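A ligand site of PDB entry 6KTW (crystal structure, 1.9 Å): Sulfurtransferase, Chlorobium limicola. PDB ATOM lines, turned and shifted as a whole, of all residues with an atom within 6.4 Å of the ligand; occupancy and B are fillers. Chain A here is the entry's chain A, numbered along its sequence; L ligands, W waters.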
ATOM      1  N   TYR A 191     -13.058  -1.191   9.849  1.00  0.00           N
ATOM      2  CA  TYR A 191     -13.040  -1.716  11.201  1.00  0.00           C
ATOM      3  C   TYR A 191     -13.236  -3.242  11.162  1.00  0.00           C
ATOM      4  O   TYR A 191     -14.346  -3.716  10.852  1.00  0.00           O
ATOM      5  CB  TYR A 191     -14.119  -1.050  12.054  1.00  0.00           C
ATOM      6  CG  TYR A 191     -14.294  -1.678  13.411  1.00  0.00           C
ATOM      7  CD1 TYR A 191     -13.192  -1.947  14.235  1.00  0.00           C
ATOM      8  CD2 TYR A 191     -15.563  -1.961  13.898  1.00  0.00           C
ATOM      9  CE1 TYR A 191     -13.374  -2.500  15.544  1.00  0.00           C
ATOM     10  CE2 TYR A 191     -15.760  -2.481  15.167  1.00  0.00           C
ATOM     11  CZ  TYR A 191     -14.681  -2.772  15.972  1.00  0.00           C
ATOM     12  OH  TYR A 191     -14.967  -3.305  17.224  1.00  0.00           O
ATOM     13  N   THR A 210      -8.918   0.029  11.478  1.00  0.00           N
ATOM     14  CA  THR A 210      -8.908   1.115  12.453  1.00  0.00           C
ATOM     15  C   THR A 210      -8.328   0.683  13.796  1.00  0.00           C
ATOM     16  O   THR A 210      -7.811   1.530  14.543  1.00  0.00           O
ATOM     17  CB  THR A 210     -10.332   1.662  12.673  1.00  0.00           C
ATOM     18  OG1 THR A 210     -11.215   0.565  12.991  1.00  0.00           O
ATOM     19  CG2 THR A 210     -10.884   2.297  11.380  1.00  0.00           C
ATOM     20  N   LEU A 211      -8.406  -0.505  14.183  1.00  0.00           N
ATOM     21  CA  LEU A 211      -7.692  -1.095  15.317  1.00  0.00           C
ATOM     22  C   LEU A 211      -6.170  -0.910  15.156  1.00  0.00           C
ATOM     23  O   LEU A 211      -5.432  -1.111  16.120  1.00  0.00           O
ATOM     24  CB  LEU A 211      -8.037  -2.573  15.450  1.00  0.00           C
ATOM     25  CG  LEU A 211      -9.493  -2.903  15.807  1.00  0.00           C
ATOM     26  CD1 LEU A 211      -9.722  -4.404  15.769  1.00  0.00           C
ATOM     27  CD2 LEU A 211      -9.858  -2.329  17.163  1.00  0.00           C
ATOM     28  N   GLU A 214      -6.330   2.840  16.946  1.00  0.00           N
ATOM     29  CA  GLU A 214      -7.077   3.080  18.182  1.00  0.00           C
ATOM     30  C   GLU A 214      -7.232   1.772  18.984  1.00  0.00           C
ATOM     31  O   GLU A 214      -7.294   0.682  18.426  1.00  0.00           O
ATOM     32  CB  GLU A 214      -8.468   3.705  17.936  1.00  0.00           C
ATOM     33  CG  GLU A 214      -9.397   2.844  17.164  1.00  0.00           C
ATOM     34  CD  GLU A 214     -10.737   3.557  16.847  1.00  0.00           C
ATOM     35  OE1 GLU A 214     -10.905   4.755  17.191  1.00  0.00           O
ATOM     36  OE2 GLU A 214     -11.646   2.914  16.247  1.00  0.00           O
ATOM     37  N   TRP A 219     -11.164   2.764  23.241  1.00  0.00           N
ATOM     38  CA  TRP A 219     -11.596   3.355  21.968  1.00  0.00           C
ATOM     39  C   TRP A 219     -11.010   4.758  21.768  1.00  0.00           C
ATOM     40  O   TRP A 219     -11.562   5.605  21.038  1.00  0.00           O
ATOM     41  CB  TRP A 219     -13.119   3.329  21.791  1.00  0.00           C
ATOM     42  CG  TRP A 219     -13.622   1.886  21.743  1.00  0.00           C
ATOM     43  CD1 TRP A 219     -14.530   1.298  22.574  1.00  0.00           C
ATOM     44  CD2 TRP A 219     -13.263   0.880  20.775  1.00  0.00           C
ATOM     45  NE1 TRP A 219     -14.753  -0.002  22.204  1.00  0.00           N
ATOM     46  CE2 TRP A 219     -13.972  -0.294  21.121  1.00  0.00           C
ATOM     47  CE3 TRP A 219     -12.376   0.841  19.691  1.00  0.00           C
ATOM     48  CZ2 TRP A 219     -13.821  -1.484  20.405  1.00  0.00           C
ATOM     49  CZ3 TRP A 219     -12.232  -0.361  18.980  1.00  0.00           C
ATOM     50  CH2 TRP A 219     -12.968  -1.500  19.335  1.00  0.00           C
ATOM     51  N   PHE A 257     -21.072  -5.851  14.736  1.00  0.00           N
ATOM     52  CA  PHE A 257     -20.136  -4.734  14.503  1.00  0.00           C
ATOM     53  C   PHE A 257     -20.669  -3.897  13.344  1.00  0.00           C
ATOM     54  O   PHE A 257     -20.187  -4.028  12.205  1.00  0.00           O
ATOM     55  CB  PHE A 257     -18.724  -5.244  14.201  1.00  0.00           C
ATOM     56  CG  PHE A 257     -18.165  -6.121  15.300  1.00  0.00           C
ATOM     57  CD1 PHE A 257     -17.852  -5.578  16.556  1.00  0.00           C
ATOM     58  CD2 PHE A 257     -17.993  -7.476  15.087  1.00  0.00           C
ATOM     59  CE1 PHE A 257     -17.338  -6.396  17.601  1.00  0.00           C
ATOM     60  CE2 PHE A 257     -17.470  -8.300  16.110  1.00  0.00           C
ATOM     61  CZ  PHE A 257     -17.158  -7.747  17.367  1.00  0.00           C
ATOM     62  N   PRO A 258     -21.667  -3.037  13.585  1.00  0.00           N
ATOM     63  CA  PRO A 258     -22.124  -2.173  12.479  1.00  0.00           C
ATOM     64  C   PRO A 258     -21.021  -1.269  11.934  1.00  0.00           C
ATOM     65  O   PRO A 258     -21.066  -0.891  10.761  1.00  0.00           O
ATOM     66  CB  PRO A 258     -23.278  -1.360  13.093  1.00  0.00           C
ATOM     67  CG  PRO A 258     -23.721  -2.172  14.325  1.00  0.00           C
ATOM     68  CD  PRO A 258     -22.409  -2.788  14.830  1.00  0.00           C
ATOM     69  N   GLY A 259     -19.999  -0.958  12.745  1.00  0.00           N
ATOM     70  CA  GLY A 259     -18.925  -0.095  12.250  1.00  0.00           C
ATOM     71  C   GLY A 259     -18.114  -0.704  11.137  1.00  0.00           C
ATOM     72  O   GLY A 259     -17.460   0.037  10.380  1.00  0.00           O
ATOM     73  N   SER A 260     -18.134  -2.039  11.002  1.00  0.00           N
ATOM     74  CA  SER A 260     -17.447  -2.702   9.914  1.00  0.00           C
ATOM     75  C   SER A 260     -17.976  -2.281   8.567  1.00  0.00           C
ATOM     76  O   SER A 260     -17.316  -2.528   7.544  1.00  0.00           O
ATOM     77  CB  SER A 260     -17.569  -4.237  10.060  1.00  0.00           C
ATOM     78  OG  SER A 260     -16.829  -4.670  11.195  1.00  0.00           O
ATOM     79  N   ALA A 262     -19.314   1.012   8.154  1.00  0.00           N
ATOM     80  CA  ALA A 262     -19.232   2.484   8.054  1.00  0.00           C
ATOM     81  C   ALA A 262     -17.799   2.909   7.714  1.00  0.00           C
ATOM     82  O   ALA A 262     -17.164   3.656   8.445  1.00  0.00           O
ATOM     83  CB  ALA A 262     -19.723   3.136   9.344  1.00  0.00           C
ATOM     84  N   ILE A 265     -16.577   6.796   7.471  1.00  0.00           N
ATOM     85  CA  ILE A 265     -16.372   7.449   8.774  1.00  0.00           C
ATOM     86  C   ILE A 265     -15.054   6.967   9.361  1.00  0.00           C
ATOM     87  O   ILE A 265     -14.262   7.749   9.910  1.00  0.00           O
ATOM     88  CB  ILE A 265     -17.536   7.159   9.756  1.00  0.00           C
ATOM     89  CG1 ILE A 265     -18.902   7.519   9.184  1.00  0.00           C
ATOM     90  CG2 ILE A 265     -17.342   8.037  11.036  1.00  0.00           C
ATOM     91  CD1 ILE A 265     -20.085   7.032  10.083  1.00  0.00           C
ATOM     92  N   GLY A 355     -26.655   4.175  21.846  1.00  0.00           N
ATOM     93  CA  GLY A 355     -26.039   4.251  20.516  1.00  0.00           C
ATOM     94  C   GLY A 355     -25.253   3.020  20.095  1.00  0.00           C
ATOM     95  O   GLY A 355     -24.970   2.862  18.912  1.00  0.00           O
ATOM     96  N   TYR A 356     -24.894   2.158  21.034  1.00  0.00           N
ATOM     97  CA  TYR A 356     -23.869   1.155  20.749  1.00  0.00           C
ATOM     98  C   TYR A 356     -24.202  -0.135  21.501  1.00  0.00           C
ATOM     99  O   TYR A 356     -24.617  -0.077  22.652  1.00  0.00           O
ATOM    100  CB  TYR A 356     -22.504   1.620  21.239  1.00  0.00           C
ATOM    101  CG  TYR A 356     -21.962   2.882  20.588  1.00  0.00           C
ATOM    102  CD1 TYR A 356     -22.408   4.149  21.001  1.00  0.00           C
ATOM    103  CD2 TYR A 356     -21.019   2.791  19.588  1.00  0.00           C
ATOM    104  CE1 TYR A 356     -21.893   5.297  20.427  1.00  0.00           C
ATOM    105  CE2 TYR A 356     -20.468   3.958  18.984  1.00  0.00           C
ATOM    106  CZ  TYR A 356     -20.911   5.194  19.408  1.00  0.00           C
ATOM    107  OH  TYR A 356     -20.391   6.340  18.855  1.00  0.00           O
ATOM    108  N   TYR A 358     -22.288  -2.084  22.952  1.00  0.00           N
ATOM    109  CA  TYR A 358     -21.307  -2.336  24.003  1.00  0.00           C
ATOM    110  C   TYR A 358     -21.280  -1.212  25.027  1.00  0.00           C
ATOM    111  O   TYR A 358     -20.356  -1.151  25.834  1.00  0.00           O
ATOM    112  CB  TYR A 358     -19.895  -2.550  23.423  1.00  0.00           C
ATOM    113  CG  TYR A 358     -19.447  -1.414  22.490  1.00  0.00           C
ATOM    114  CD1 TYR A 358     -18.755  -0.318  22.999  1.00  0.00           C
ATOM    115  CD2 TYR A 358     -19.691  -1.474  21.116  1.00  0.00           C
ATOM    116  CE1 TYR A 358     -18.349   0.740  22.153  1.00  0.00           C
ATOM    117  CE2 TYR A 358     -19.288  -0.424  20.247  1.00  0.00           C
ATOM    118  CZ  TYR A 358     -18.598   0.669  20.783  1.00  0.00           C
ATOM    119  OH  TYR A 358     -18.180   1.725  19.967  1.00  0.00           O
ATOM    120  N   ALA A 377     -25.618   5.897  15.423  1.00  0.00           N
ATOM    121  CA  ALA A 377     -24.175   6.057  15.559  1.00  0.00           C
ATOM    122  C   ALA A 377     -23.406   5.704  14.281  1.00  0.00           C
ATOM    123  O   ALA A 377     -22.200   5.988  14.233  1.00  0.00           O
ATOM    124  CB  ALA A 377     -23.640   5.199  16.730  1.00  0.00           C
ATOM    125  N   TYR A 378     -24.045   5.089  13.280  1.00  0.00           N
ATOM    126  CA  TYR A 378     -23.326   4.603  12.110  1.00  0.00           C
ATOM    127  C   TYR A 378     -23.714   5.336  10.823  1.00  0.00           C
ATOM    128  O   TYR A 378     -23.417   4.833   9.727  1.00  0.00           O
ATOM    129  CB  TYR A 378     -23.531   3.079  11.949  1.00  0.00           C
ATOM    130  CG  TYR A 378     -23.029   2.391  13.182  1.00  0.00           C
ATOM    131  CD1 TYR A 378     -21.656   2.218  13.369  1.00  0.00           C
ATOM    132  CD2 TYR A 378     -23.926   2.018  14.206  1.00  0.00           C
ATOM    133  CE1 TYR A 378     -21.161   1.618  14.540  1.00  0.00           C
ATOM    134  CE2 TYR A 378     -23.427   1.426  15.400  1.00  0.00           C
ATOM    135  CZ  TYR A 378     -22.042   1.237  15.565  1.00  0.00           C
ATOM    136  OH  TYR A 378     -21.536   0.659  16.739  1.00  0.00           O
ATOM    137  N   HIS A 379     -24.426   6.439  10.941  1.00  0.00           N
ATOM    138  CA  HIS A 379     -24.859   7.258   9.817  1.00  0.00           C
ATOM    139  C   HIS A 379     -24.612   8.734  10.112  1.00  0.00           C
ATOM    140  O   HIS A 379     -24.898   9.217  11.213  1.00  0.00           O
ATOM    141  CB  HIS A 379     -26.351   7.005   9.529  1.00  0.00           C
ATOM    142  CG  HIS A 379     -26.641   5.603   9.062  1.00  0.00           C
ATOM    143  ND1 HIS A 379     -26.755   4.538   9.940  1.00  0.00           N
ATOM    144  CD2 HIS A 379     -26.750   5.082   7.819  1.00  0.00           C
ATOM    145  CE1 HIS A 379     -26.943   3.422   9.253  1.00  0.00           C
ATOM    146  NE2 HIS A 379     -26.941   3.719   7.967  1.00  0.00           N
ATOM    147  N   CYS A 415     -18.266  12.094  20.195  1.00  0.00           N
ATOM    148  CA  CYS A 415     -19.505  11.349  20.125  1.00  0.00           C
ATOM    149  C   CYS A 415     -19.448  10.195  21.137  1.00  0.00           C
ATOM    150  O   CYS A 415     -19.029  10.389  22.301  1.00  0.00           O
ATOM    151  CB  CYS A 415     -19.755  10.881  18.648  1.00  0.00           C
ATOM    152  SG  CYS A 415     -18.565   9.630  17.989  1.00  0.00           S
ATOM    153  N   GLY A 416     -19.833   8.995  20.729  1.00  0.00           N
ATOM    154  CA  GLY A 416     -19.743   7.876  21.662  1.00  0.00           C
ATOM    155  C   GLY A 416     -18.303   7.535  21.992  1.00  0.00           C
ATOM    156  O   GLY A 416     -17.907   7.489  23.166  1.00  0.00           O
ATOM    157  N   THR A 417     -17.480   7.317  20.951  1.00  0.00           N
ATOM    158  CA  THR A 417     -16.064   7.010  21.118  1.00  0.00           C
ATOM    159  C   THR A 417     -15.179   7.792  20.159  1.00  0.00           C
ATOM    160  O   THR A 417     -13.959   7.573  20.162  1.00  0.00           O
ATOM    161  CB  THR A 417     -15.759   5.523  20.915  1.00  0.00           C
ATOM    162  OG1 THR A 417     -15.774   5.219  19.501  1.00  0.00           O
ATOM    163  CG2 THR A 417     -16.771   4.631  21.670  1.00  0.00           C
ATOM    164  N   GLY A 418     -15.738   8.699  19.343  1.00  0.00           N
ATOM    165  CA  GLY A 418     -14.905   9.632  18.591  1.00  0.00           C
ATOM    166  C   GLY A 418     -14.958   9.519  17.062  1.00  0.00           C
ATOM    167  O   GLY A 418     -14.357  10.367  16.372  1.00  0.00           O
ATOM    168  N   TRP A 419     -15.637   8.535  16.476  1.00  0.00           N
ATOM    169  CA  TRP A 419     -15.651   8.452  15.005  1.00  0.00           C
ATOM    170  C   TRP A 419     -16.435   9.605  14.393  1.00  0.00           C
ATOM    171  O   TRP A 419     -15.963  10.257  13.451  1.00  0.00           O
ATOM    172  CB  TRP A 419     -16.272   7.138  14.547  1.00  0.00           C
ATOM    173  CG  TRP A 419     -15.314   6.014  14.512  1.00  0.00           C
ATOM    174  CD1 TRP A 419     -14.249   5.777  15.366  1.00  0.00           C
ATOM    175  CD2 TRP A 419     -15.301   4.962  13.544  1.00  0.00           C
ATOM    176  NE1 TRP A 419     -13.604   4.589  14.995  1.00  0.00           N
ATOM    177  CE2 TRP A 419     -14.211   4.096  13.862  1.00  0.00           C
ATOM    178  CE3 TRP A 419     -16.107   4.668  12.439  1.00  0.00           C
ATOM    179  CZ2 TRP A 419     -13.935   2.961  13.106  1.00  0.00           C
ATOM    180  CZ3 TRP A 419     -15.821   3.514  11.690  1.00  0.00           C
ATOM    181  CH2 TRP A 419     -14.746   2.685  12.018  1.00  0.00           C
ATOM    182  N   ARG A 420     -17.669   9.810  14.866  1.00  0.00           N
ATOM    183  CA  ARG A 420     -18.495  10.895  14.341  1.00  0.00           C
ATOM    184  C   ARG A 420     -17.929  12.238  14.741  1.00  0.00           C
ATOM    185  O   ARG A 420     -17.964  13.177  13.947  1.00  0.00           O
ATOM    186  CB  ARG A 420     -19.911  10.747  14.868  1.00  0.00           C
ATOM    187  CG  ARG A 420     -20.595   9.463  14.408  1.00  0.00           C
ATOM    188  CD  ARG A 420     -21.979   9.363  15.101  1.00  0.00           C
ATOM    189  NE  ARG A 420     -21.738   8.832  16.465  1.00  0.00           N
ATOM    190  CZ  ARG A 420     -22.715   8.733  17.381  1.00  0.00           C
ATOM    191  NH1 ARG A 420     -23.956   9.126  17.068  1.00  0.00           N
ATOM    192  NH2 ARG A 420     -22.474   8.208  18.603  1.00  0.00           N
HETATM  193  C1  LIG L   1     -14.727   2.477  17.933  1.00  0.00           C
HETATM  194  C2  LIG L   1     -15.888   0.270  18.193  1.00  0.00           C
HETATM  195  C3  LIG L   1     -14.890   1.028  15.968  1.00  0.00           C
HETATM  196  O1  LIG L   1     -19.126   1.190  17.252  1.00  0.00           O
HETATM  197  O2  LIG L   1     -17.843   0.460  15.537  1.00  0.00           O
HETATM  198  C4  LIG L   1     -18.770   3.989  14.253  1.00  0.00           C
HETATM  199  C5  LIG L   1     -16.754   3.018  15.586  1.00  0.00           C
HETATM  200  N1  LIG L   1     -18.375   4.789  16.250  1.00  0.00           N
HETATM  201  N2  LIG L   1     -19.759   4.959  14.523  1.00  0.00           N
HETATM  202  C6  LIG L   1     -18.139   1.153  16.564  1.00  0.00           C
HETATM  203  C7  LIG L   1     -17.919   3.905  15.343  1.00  0.00           C
HETATM  204  C8  LIG L   1     -19.478   5.465  15.793  1.00  0.00           C
HETATM  205  C9  LIG L   1     -16.966   2.208  16.874  1.00  0.00           C
HETATM  206  N3  LIG L   1     -15.615   1.482  17.233  1.00  0.00           N
HETATM  207  O   HOH W   1     -17.303  -2.721  18.433  1.00  0.00           O
HETATM  208  O   HOH W   2     -13.099   5.152  18.546  1.00  0.00           O
HETATM  209  O   HOH W   3     -17.662   6.373  17.996  1.00  0.00           O
HETATM  210  O   HOH W   4     -19.177  -1.783  15.320  1.00  0.00           O
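The side-chain hydroxyl of Tyr 378 sits at hydrogen-bond distance from an oxygen (O1) of the ligand (2.5 Å).
O of Ala 377 sits close to N2 of the ligand, at 2.7 Å.
O1 of the ligand sits at hydrogen-bond distance from OH of Tyr 358 (2.9 Å).
Water W3 lies within hydrogen-bond range of N1 of the ligand (2.5 Å), OG1 of Thr 417 (2.7 Å), OH of Tyr 356 (2.9 Å), N of Gly 418 (3.3 Å), N of Trp 419 (3.3 Å) and SG of Cys 415 (3.4 Å).
Water W4 lies within hydrogen-bond range of O2 of the ligand (2.6 Å) and N of Gly 259 (2.8 Å).
Water W2 lies within hydrogen-bond range of OE1 of Glu 214 (2.6 Å) and OG1 of Thr 417 (2.8 Å).
Tyr 191 touches the ligand.
Glu 214 touches the ligand (OE2 to C1, 3.5 Å).
Trp 219 touches the ligand.
Gly 259 touches the ligand.
Tyr 356 touches the ligand (OH to C8, 3.3 Å).
Thr 417 touches the ligand.
Trp 419 touches the ligand (CD2 to C5, 3.2 Å).
Hydrophobic or aromatic side chains that line the ligand: Tyr 191, Trp 219, Tyr 356, Tyr 358, Tyr 378 and Trp 419.
Within 4 Å of the ligand: Tyr 191, Glu 214, Trp 219, Gly 259, Tyr 356, Tyr 358, Ala 377, Tyr 378, Thr 417 and Trp 419.
The nearest printed residue that does not touch the ligand is Arg 420 (4.1 Å).
The indole nitrogen of Trp 419 is in hydrogen-bond range of the side-chain carboxylate of Glu 214, at 2.9 Å.
N of Trp 419 is in hydrogen-bond range of SG of Cys 415.
NH2 of Arg 420 sits at hydrogen-bond distance from OH of Tyr 356 (2.8 Å).
OH of Tyr 356 lies close to N of Gly 416 (3.3 Å).
O of Tyr 191 sits at hydrogen-bond distance from OG of Ser 260 (2.7 Å).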
